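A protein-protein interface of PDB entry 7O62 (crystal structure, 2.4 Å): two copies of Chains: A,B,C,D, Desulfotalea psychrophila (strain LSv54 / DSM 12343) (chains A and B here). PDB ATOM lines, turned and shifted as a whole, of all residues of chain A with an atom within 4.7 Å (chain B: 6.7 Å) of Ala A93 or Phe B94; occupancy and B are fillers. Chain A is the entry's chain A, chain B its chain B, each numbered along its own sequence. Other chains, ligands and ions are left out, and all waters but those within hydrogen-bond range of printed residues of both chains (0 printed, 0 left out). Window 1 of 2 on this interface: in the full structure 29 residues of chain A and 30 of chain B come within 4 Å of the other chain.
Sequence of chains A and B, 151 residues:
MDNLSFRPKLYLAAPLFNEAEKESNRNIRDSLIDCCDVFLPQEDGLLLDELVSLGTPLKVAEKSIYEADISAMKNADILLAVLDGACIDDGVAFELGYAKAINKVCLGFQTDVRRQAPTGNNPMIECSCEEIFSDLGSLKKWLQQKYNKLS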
ATOM      1  N   ILE A  88      -1.800   6.104 -14.373  1.00  0.00           N
ATOM      2  CA  ILE A  88      -2.447   6.951 -15.363  1.00  0.00           C
ATOM      3  C   ILE A  88      -3.713   7.519 -14.737  1.00  0.00           C
ATOM      4  O   ILE A  88      -4.529   6.781 -14.185  1.00  0.00           O
ATOM      5  CB  ILE A  88      -2.725   6.166 -16.655  1.00  0.00           C
ATOM      6  CG1 ILE A  88      -1.379   5.901 -17.377  1.00  0.00           C
ATOM      7  CG2 ILE A  88      -3.749   6.923 -17.548  1.00  0.00           C
ATOM      8  CD1 ILE A  88      -1.406   4.819 -18.449  1.00  0.00           C
ATOM      9  N   ASP A  89      -3.866   8.839 -14.769  1.00  0.00           N
ATOM     10  CA  ASP A  89      -4.992   9.443 -14.071  1.00  0.00           C
ATOM     11  C   ASP A  89      -6.318   8.873 -14.573  1.00  0.00           C
ATOM     12  O   ASP A  89      -6.535   8.709 -15.785  1.00  0.00           O
ATOM     13  CB  ASP A  89      -4.978  10.957 -14.244  1.00  0.00           C
ATOM     14  CG  ASP A  89      -6.208  11.615 -13.633  1.00  0.00           C
ATOM     15  OD1 ASP A  89      -7.105  12.026 -14.403  1.00  0.00           O
ATOM     16  OD2 ASP A  89      -6.289  11.711 -12.379  1.00  0.00           O
ATOM     17  N   ASP A  90      -7.220   8.563 -13.633  1.00  0.00           N
ATOM     18  CA  ASP A  90      -8.481   7.943 -14.045  1.00  0.00           C
ATOM     19  C   ASP A  90      -9.380   8.932 -14.774  1.00  0.00           C
ATOM     20  O   ASP A  90     -10.175   8.524 -15.627  1.00  0.00           O
ATOM     21  CB  ASP A  90      -9.222   7.343 -12.856  1.00  0.00           C
ATOM     22  CG  ASP A  90      -9.298   8.278 -11.698  1.00  0.00           C
ATOM     23  OD1 ASP A  90      -8.434   9.174 -11.592  1.00  0.00           O
ATOM     24  OD2 ASP A  90     -10.237   8.138 -10.896  1.00  0.00           O
ATOM     25  N   GLY A  91      -9.283  10.224 -14.450  1.00  0.00           N
ATOM     26  CA  GLY A  91      -9.969  11.223 -15.255  1.00  0.00           C
ATOM     27  C   GLY A  91      -9.482  11.213 -16.691  1.00  0.00           C
ATOM     28  O   GLY A  91     -10.288  11.252 -17.629  1.00  0.00           O
ATOM     29  N   VAL A  92      -8.158  11.117 -16.881  1.00  0.00           N
ATOM     30  CA  VAL A  92      -7.595  11.110 -18.229  1.00  0.00           C
ATOM     31  C   VAL A  92      -8.063   9.887 -18.995  1.00  0.00           C
ATOM     32  O   VAL A  92      -8.509   9.984 -20.146  1.00  0.00           O
ATOM     33  CB  VAL A  92      -6.060  11.168 -18.175  1.00  0.00           C
ATOM     34  CG1 VAL A  92      -5.456  10.772 -19.554  1.00  0.00           C
ATOM     35  CG2 VAL A  92      -5.635  12.553 -17.773  1.00  0.00           C
ATOM     36  N   ALA A  93      -7.974   8.717 -18.359  1.00  0.00           N
ATOM     37  CA  ALA A  93      -8.363   7.469 -19.007  1.00  0.00           C
ATOM     38  C   ALA A  93      -9.857   7.447 -19.350  1.00  0.00           C
ATOM     39  O   ALA A  93     -10.241   6.963 -20.418  1.00  0.00           O
ATOM     40  CB  ALA A  93      -7.982   6.286 -18.113  1.00  0.00           C
ATOM     41  N   PHE A  94     -10.718   7.971 -18.470  1.00  0.00           N
ATOM     42  CA  PHE A  94     -12.125   8.129 -18.847  1.00  0.00           C
ATOM     43  C   PHE A  94     -12.255   8.962 -20.127  1.00  0.00           C
ATOM     44  O   PHE A  94     -12.890   8.536 -21.105  1.00  0.00           O
ATOM     45  CB  PHE A  94     -12.913   8.777 -17.703  1.00  0.00           C
ATOM     46  CG  PHE A  94     -14.387   9.010 -18.014  1.00  0.00           C
ATOM     47  CD1 PHE A  94     -15.358   8.163 -17.497  1.00  0.00           C
ATOM     48  CD2 PHE A  94     -14.796  10.090 -18.796  1.00  0.00           C
ATOM     49  CE1 PHE A  94     -16.696   8.357 -17.774  1.00  0.00           C
ATOM     50  CE2 PHE A  94     -16.137  10.303 -19.073  1.00  0.00           C
ATOM     51  CZ  PHE A  94     -17.099   9.433 -18.563  1.00  0.00           C
ATOM     52  N   GLU A  95     -11.634  10.148 -20.147  1.00  0.00           N
ATOM     53  CA  GLU A  95     -11.791  11.055 -21.283  1.00  0.00           C
ATOM     54  C   GLU A  95     -11.294  10.408 -22.573  1.00  0.00           C
ATOM     55  O   GLU A  95     -11.892  10.591 -23.640  1.00  0.00           O
ATOM     56  CB  GLU A  95     -11.063  12.381 -20.987  1.00  0.00           C
ATOM     57  CG  GLU A  95     -11.811  13.258 -19.973  1.00  0.00           C
ATOM     58  CD  GLU A  95     -10.932  14.197 -19.163  1.00  0.00           C
ATOM     59  OE1 GLU A  95      -9.692  14.164 -19.327  1.00  0.00           O
ATOM     60  OE2 GLU A  95     -11.479  14.971 -18.337  1.00  0.00           O
ATOM     61  N   LEU A  96     -10.213   9.629 -22.497  1.00  0.00           N
ATOM     62  CA  LEU A  96      -9.715   8.946 -23.687  1.00  0.00           C
ATOM     63  C   LEU A  96     -10.760   7.966 -24.213  1.00  0.00           C
ATOM     64  O   LEU A  96     -11.135   8.004 -25.400  1.00  0.00           O
ATOM     65  CB  LEU A  96      -8.405   8.233 -23.354  1.00  0.00           C
ATOM     66  CG  LEU A  96      -7.671   7.444 -24.425  1.00  0.00           C
ATOM     67  CD1 LEU A  96      -7.384   8.311 -25.617  1.00  0.00           C
ATOM     68  CD2 LEU A  96      -6.348   6.902 -23.856  1.00  0.00           C
ATOM     69  N   GLY A  97     -11.280   7.111 -23.338  1.00  0.00           N
ATOM     70  CA  GLY A  97     -12.317   6.192 -23.782  1.00  0.00           C
ATOM     71  C   GLY A  97     -13.527   6.904 -24.364  1.00  0.00           C
ATOM     72  O   GLY A  97     -14.065   6.496 -25.407  1.00  0.00           O
ATOM     73  N   LYS A 100     -12.621   8.336 -27.689  1.00  0.00           N
ATOM     74  CA  LYS A 100     -12.375   7.297 -28.679  1.00  0.00           C
ATOM     75  C   LYS A 100     -13.687   6.734 -29.191  1.00  0.00           C
ATOM     76  O   LYS A 100     -13.872   6.591 -30.404  1.00  0.00           O
ATOM     77  CB  LYS A 100     -11.502   6.176 -28.099  1.00  0.00           C
ATOM     78  CG  LYS A 100     -11.243   5.046 -29.126  1.00  0.00           C
ATOM     79  CD  LYS A 100     -10.194   5.522 -30.169  1.00  0.00           C
ATOM     80  CE  LYS A 100      -9.933   4.453 -31.214  1.00  0.00           C
ATOM     81  NZ  LYS A 100      -9.092   5.000 -32.300  1.00  0.00           N
ATOM     82  N   MET A 124      -5.823  -1.050 -23.395  1.00  0.00           N
ATOM     83  CA  MET A 124      -6.875  -0.122 -23.777  1.00  0.00           C
ATOM     84  C   MET A 124      -6.298   1.261 -24.041  1.00  0.00           C
ATOM     85  O   MET A 124      -6.617   1.883 -25.059  1.00  0.00           O
ATOM     86  CB  MET A 124      -7.961  -0.101 -22.711  1.00  0.00           C
ATOM     87  CG  MET A 124      -8.260  -1.524 -22.293  1.00  0.00           C
ATOM     88  SD  MET A 124      -9.175  -2.513 -23.509  1.00  0.00           S
ATOM     89  CE  MET A 124     -10.374  -1.335 -24.207  1.00  0.00           C
ATOM     90  N   ILE A 125      -5.414   1.742 -23.155  1.00  0.00           N
ATOM     91  CA  ILE A 125      -4.706   2.990 -23.407  1.00  0.00           C
ATOM     92  C   ILE A 125      -3.830   2.863 -24.652  1.00  0.00           C
ATOM     93  O   ILE A 125      -3.856   3.720 -25.542  1.00  0.00           O
ATOM     94  CB  ILE A 125      -3.872   3.404 -22.184  1.00  0.00           C
ATOM     95  CG1 ILE A 125      -4.717   3.461 -20.908  1.00  0.00           C
ATOM     96  CG2 ILE A 125      -3.250   4.745 -22.430  1.00  0.00           C
ATOM     97  CD1 ILE A 125      -6.007   4.321 -21.052  1.00  0.00           C
ATOM     98  N   SER A 128      -5.745   2.516 -27.953  1.00  0.00           N
ATOM     99  CA  SER A 128      -6.690   3.542 -28.346  1.00  0.00           C
ATOM    100  C   SER A 128      -5.995   4.812 -28.811  1.00  0.00           C
ATOM    101  O   SER A 128      -6.558   5.541 -29.628  1.00  0.00           O
ATOM    102  CB  SER A 128      -7.680   3.819 -27.206  1.00  0.00           C
ATOM    103  OG  SER A 128      -7.042   4.395 -26.074  1.00  0.00           O
ATOM    104  N   TYR B  66      -7.827  -5.791 -26.820  1.00  0.00           N
ATOM    105  CA  TYR B  66      -8.551  -4.544 -27.044  1.00  0.00           C
ATOM    106  C   TYR B  66      -9.863  -4.764 -27.788  1.00  0.00           C
ATOM    107  O   TYR B  66     -10.931  -4.367 -27.321  1.00  0.00           O
ATOM    108  CB  TYR B  66      -7.653  -3.595 -27.823  1.00  0.00           C
ATOM    109  CG  TYR B  66      -8.229  -2.226 -28.111  1.00  0.00           C
ATOM    110  CD1 TYR B  66      -8.298  -1.245 -27.111  1.00  0.00           C
ATOM    111  CD2 TYR B  66      -8.660  -1.893 -29.394  1.00  0.00           C
ATOM    112  CE1 TYR B  66      -8.789   0.022 -27.386  1.00  0.00           C
ATOM    113  CE2 TYR B  66      -9.163  -0.642 -29.677  1.00  0.00           C
ATOM    114  CZ  TYR B  66      -9.216   0.314 -28.684  1.00  0.00           C
ATOM    115  OH  TYR B  66      -9.709   1.552 -28.995  1.00  0.00           O
ATOM    116  N   ILE B  70     -13.807  -4.309 -26.644  1.00  0.00           N
ATOM    117  CA  ILE B  70     -14.690  -3.329 -27.279  1.00  0.00           C
ATOM    118  C   ILE B  70     -15.995  -4.000 -27.703  1.00  0.00           C
ATOM    119  O   ILE B  70     -17.085  -3.546 -27.342  1.00  0.00           O
ATOM    120  CB  ILE B  70     -13.980  -2.638 -28.464  1.00  0.00           C
ATOM    121  CG1 ILE B  70     -12.674  -1.966 -28.015  1.00  0.00           C
ATOM    122  CG2 ILE B  70     -14.891  -1.580 -29.146  1.00  0.00           C
ATOM    123  CD1 ILE B  70     -12.856  -0.577 -27.450  1.00  0.00           C
ATOM    124  N   MET B  73     -18.145  -4.820 -24.681  1.00  0.00           N
ATOM    125  CA  MET B  73     -18.804  -3.602 -24.231  1.00  0.00           C
ATOM    126  C   MET B  73     -19.951  -3.242 -25.162  1.00  0.00           C
ATOM    127  O   MET B  73     -21.049  -2.892 -24.708  1.00  0.00           O
ATOM    128  CB  MET B  73     -17.790  -2.445 -24.141  1.00  0.00           C
ATOM    129  CG  MET B  73     -16.870  -2.501 -22.914  1.00  0.00           C
ATOM    130  SD  MET B  73     -15.672  -1.118 -22.919  1.00  0.00           S
ATOM    131  CE  MET B  73     -16.760   0.247 -23.218  1.00  0.00           C
ATOM    132  N   ASP B  89      -8.202   1.680 -11.730  1.00  0.00           N
ATOM    133  CA  ASP B  89      -7.409   1.124 -12.826  1.00  0.00           C
ATOM    134  C   ASP B  89      -7.660   1.886 -14.132  1.00  0.00           C
ATOM    135  O   ASP B  89      -8.784   2.298 -14.419  1.00  0.00           O
ATOM    136  CB  ASP B  89      -7.760  -0.342 -13.010  1.00  0.00           C
ATOM    137  CG  ASP B  89      -7.100  -0.933 -14.223  1.00  0.00           C
ATOM    138  OD1 ASP B  89      -7.827  -1.261 -15.182  1.00  0.00           O
ATOM    139  OD2 ASP B  89      -5.845  -1.046 -14.235  1.00  0.00           O
ATOM    140  N   ASP B  90      -6.629   2.042 -14.965  1.00  0.00           N
ATOM    141  CA  ASP B  90      -6.873   2.903 -16.118  1.00  0.00           C
ATOM    142  C   ASP B  90      -7.698   2.188 -17.174  1.00  0.00           C
ATOM    143  O   ASP B  90      -8.556   2.813 -17.814  1.00  0.00           O
ATOM    144  CB  ASP B  90      -5.571   3.422 -16.723  1.00  0.00           C
ATOM    145  CG  ASP B  90      -4.518   2.376 -16.841  1.00  0.00           C
ATOM    146  OD1 ASP B  90      -3.971   1.870 -15.849  1.00  0.00           O
ATOM    147  OD2 ASP B  90      -4.210   2.051 -17.985  1.00  0.00           O
ATOM    148  N   GLY B  91      -7.457   0.885 -17.371  1.00  0.00           N
ATOM    149  CA  GLY B  91      -8.342   0.098 -18.227  1.00  0.00           C
ATOM    150  C   GLY B  91      -9.804   0.255 -17.843  1.00  0.00           C
ATOM    151  O   GLY B  91     -10.666   0.533 -18.694  1.00  0.00           O
ATOM    152  N   VAL B  92     -10.100   0.145 -16.545  1.00  0.00           N
ATOM    153  CA  VAL B  92     -11.492   0.288 -16.110  1.00  0.00           C
ATOM    154  C   VAL B  92     -12.035   1.677 -16.465  1.00  0.00           C
ATOM    155  O   VAL B  92     -13.170   1.811 -16.947  1.00  0.00           O
ATOM    156  CB  VAL B  92     -11.617   0.015 -14.596  1.00  0.00           C
ATOM    157  CG1 VAL B  92     -13.012   0.439 -14.112  1.00  0.00           C
ATOM    158  CG2 VAL B  92     -11.331  -1.454 -14.260  1.00  0.00           C
ATOM    159  N   ALA B  93     -11.243   2.736 -16.190  1.00  0.00           N
ATOM    160  CA  ALA B  93     -11.700   4.103 -16.446  1.00  0.00           C
ATOM    161  C   ALA B  93     -11.947   4.327 -17.930  1.00  0.00           C
ATOM    162  O   ALA B  93     -12.959   4.916 -18.325  1.00  0.00           O
ATOM    163  CB  ALA B  93     -10.672   5.115 -15.929  1.00  0.00           C
ATOM    164  N   PHE B  94     -11.010   3.891 -18.764  1.00  0.00           N
ATOM    165  CA  PHE B  94     -11.216   3.973 -20.197  1.00  0.00           C
ATOM    166  C   PHE B  94     -12.520   3.281 -20.579  1.00  0.00           C
ATOM    167  O   PHE B  94     -13.331   3.833 -21.332  1.00  0.00           O
ATOM    168  CB  PHE B  94     -10.024   3.362 -20.933  1.00  0.00           C
ATOM    169  CG  PHE B  94     -10.217   3.256 -22.413  1.00  0.00           C
ATOM    170  CD1 PHE B  94      -9.595   4.164 -23.268  1.00  0.00           C
ATOM    171  CD2 PHE B  94     -11.006   2.255 -22.968  1.00  0.00           C
ATOM    172  CE1 PHE B  94      -9.762   4.092 -24.645  1.00  0.00           C
ATOM    173  CE2 PHE B  94     -11.184   2.173 -24.354  1.00  0.00           C
ATOM    174  CZ  PHE B  94     -10.565   3.097 -25.196  1.00  0.00           C
ATOM    175  N   GLU B  95     -12.728   2.067 -20.076  1.00  0.00           N
ATOM    176  CA  GLU B  95     -13.901   1.296 -20.466  1.00  0.00           C
ATOM    177  C   GLU B  95     -15.177   1.975 -19.979  1.00  0.00           C
ATOM    178  O   GLU B  95     -16.184   2.015 -20.705  1.00  0.00           O
ATOM    179  CB  GLU B  95     -13.785  -0.145 -19.947  1.00  0.00           C
ATOM    180  CG  GLU B  95     -12.878  -1.009 -20.839  1.00  0.00           C
ATOM    181  CD  GLU B  95     -12.494  -2.368 -20.223  1.00  0.00           C
ATOM    182  OE1 GLU B  95     -11.884  -3.207 -20.965  1.00  0.00           O
ATOM    183  OE2 GLU B  95     -12.794  -2.606 -19.024  1.00  0.00           O
ATOM    184  N   LEU B  96     -15.119   2.562 -18.778  1.00  0.00           N
ATOM    185  CA  LEU B  96     -16.242   3.321 -18.243  1.00  0.00           C
ATOM    186  C   LEU B  96     -16.597   4.500 -19.149  1.00  0.00           C
ATOM    187  O   LEU B  96     -17.777   4.760 -19.419  1.00  0.00           O
ATOM    188  CB  LEU B  96     -15.894   3.807 -16.835  1.00  0.00           C
ATOM    189  CG  LEU B  96     -16.898   4.763 -16.209  1.00  0.00           C
ATOM    190  CD1 LEU B  96     -18.317   4.173 -16.259  1.00  0.00           C
ATOM    191  CD2 LEU B  96     -16.494   5.157 -14.790  1.00  0.00           C
ATOM    192  N   GLY B  97     -15.584   5.208 -19.652  1.00  0.00           N
ATOM    193  CA  GLY B  97     -15.858   6.354 -20.504  1.00  0.00           C
ATOM    194  C   GLY B  97     -16.336   5.941 -21.881  1.00  0.00           C
ATOM    195  O   GLY B  97     -17.202   6.592 -22.472  1.00  0.00           O
ATOM    196  N   TYR B  98     -15.797   4.843 -22.399  1.00  0.00           N
ATOM    197  CA  TYR B  98     -16.256   4.353 -23.686  1.00  0.00           C
ATOM    198  C   TYR B  98     -17.724   3.935 -23.603  1.00  0.00           C
ATOM    199  O   TYR B  98     -18.544   4.323 -24.442  1.00  0.00           O
ATOM    200  CB  TYR B  98     -15.344   3.212 -24.142  1.00  0.00           C
ATOM    201  CG  TYR B  98     -15.493   2.814 -25.607  1.00  0.00           C
ATOM    202  CD1 TYR B  98     -14.538   3.165 -26.559  1.00  0.00           C
ATOM    203  CD2 TYR B  98     -16.581   2.061 -26.033  1.00  0.00           C
ATOM    204  CE1 TYR B  98     -14.688   2.791 -27.911  1.00  0.00           C
ATOM    205  CE2 TYR B  98     -16.731   1.691 -27.367  1.00  0.00           C
ATOM    206  CZ  TYR B  98     -15.788   2.052 -28.288  1.00  0.00           C
ATOM    207  OH  TYR B  98     -15.978   1.661 -29.606  1.00  0.00           O
ATOM    208  N   ALA B  99     -18.086   3.185 -22.556  1.00  0.00           N
ATOM    209  CA  ALA B  99     -19.457   2.682 -22.434  1.00  0.00           C
ATOM    210  C   ALA B  99     -20.436   3.812 -22.181  1.00  0.00           C
ATOM    211  O   ALA B  99     -21.586   3.752 -22.631  1.00  0.00           O
ATOM    212  CB  ALA B  99     -19.545   1.656 -21.301  1.00  0.00           C
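OE1 of Glu B95 lies close to SD of Met A124.
Among the printed residues, pairs that only touch across the chains: Ser A128 with Phe B94, Ala A93 with Phe B94, Ile A125 with Asp B90, Phe A94 with Ala B93, Gly A97 with Phe B94, Asp A90 with Ala B93, Phe A94 with Gly B97, Gly A97 with Tyr B98, Ser A128 with Tyr B66, Ala A93 with Asp B90, Met A124 with Tyr B66, Met A124 with Phe B94, Ala A93 with Ala B93, Lys A100 with Tyr B66, Gly A97 with Gly B97, Phe A94 with Leu B96, Ile A88 with Asp B90 and Leu A96 with Phe B94.
Printed residues of chain B that touch a printed residue of chain A: Tyr B66, Asp B90, Ala B93, Phe B94, Glu B95, Leu B96, Gly B97 and Tyr B98.
Hydrophobic or aromatic side chains of chain B that line the printed part of chain A: Tyr B66, Ala B93, Phe B94, Leu B96 and Tyr B98.
O of Met A124 is in hydrogen-bond range of OG of Ser A128, at 2.7 Å.
O of Ile A125 sits at hydrogen-bond distance from OG of Ser A128.
Asp A90 touches Ala B93, and with the chains exchanged Ala A93 touches Asp B90.
Ala A93 touches Phe B94, and with the chains exchanged Phe A94 touches Ala B93.
Phe A94 touches Leu B96, and with the chains exchanged Leu A96 touches Phe B94.
Gly A97 touches its own counterpart, Gly B97.
9 positions are printed for both chains.
Of the 19 pairs that touch across the chains among the printed residues, 10 have their exchanged pair printed and touching as well.
Ala A93 touches just these residues of chain B: Asp B90 (3.5 Å), Ala B93 (3.7 Å) and Phe B94 (3.2 Å).
Phe B94 touches just these residues of chain A: Ala A93, Leu A96, Gly A97, Met A124 and Ser A128.
Printed residues of chain B within 4 Å of Gly A97: Phe B94 (3.4 Å), Gly B97 (3.9 Å) and Tyr B98 (3.5 Å).
Printed residues of chain A within 4 Å of Tyr B66: Lys A100, Met A124 and Ser A128.
The nearest residue of chain A that does not touch Phe B94 is Phe A94 (4.1 Å).
The nearest printed residue of chain A that does not touch Asp B90 is Asp A89 (5.5 Å).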
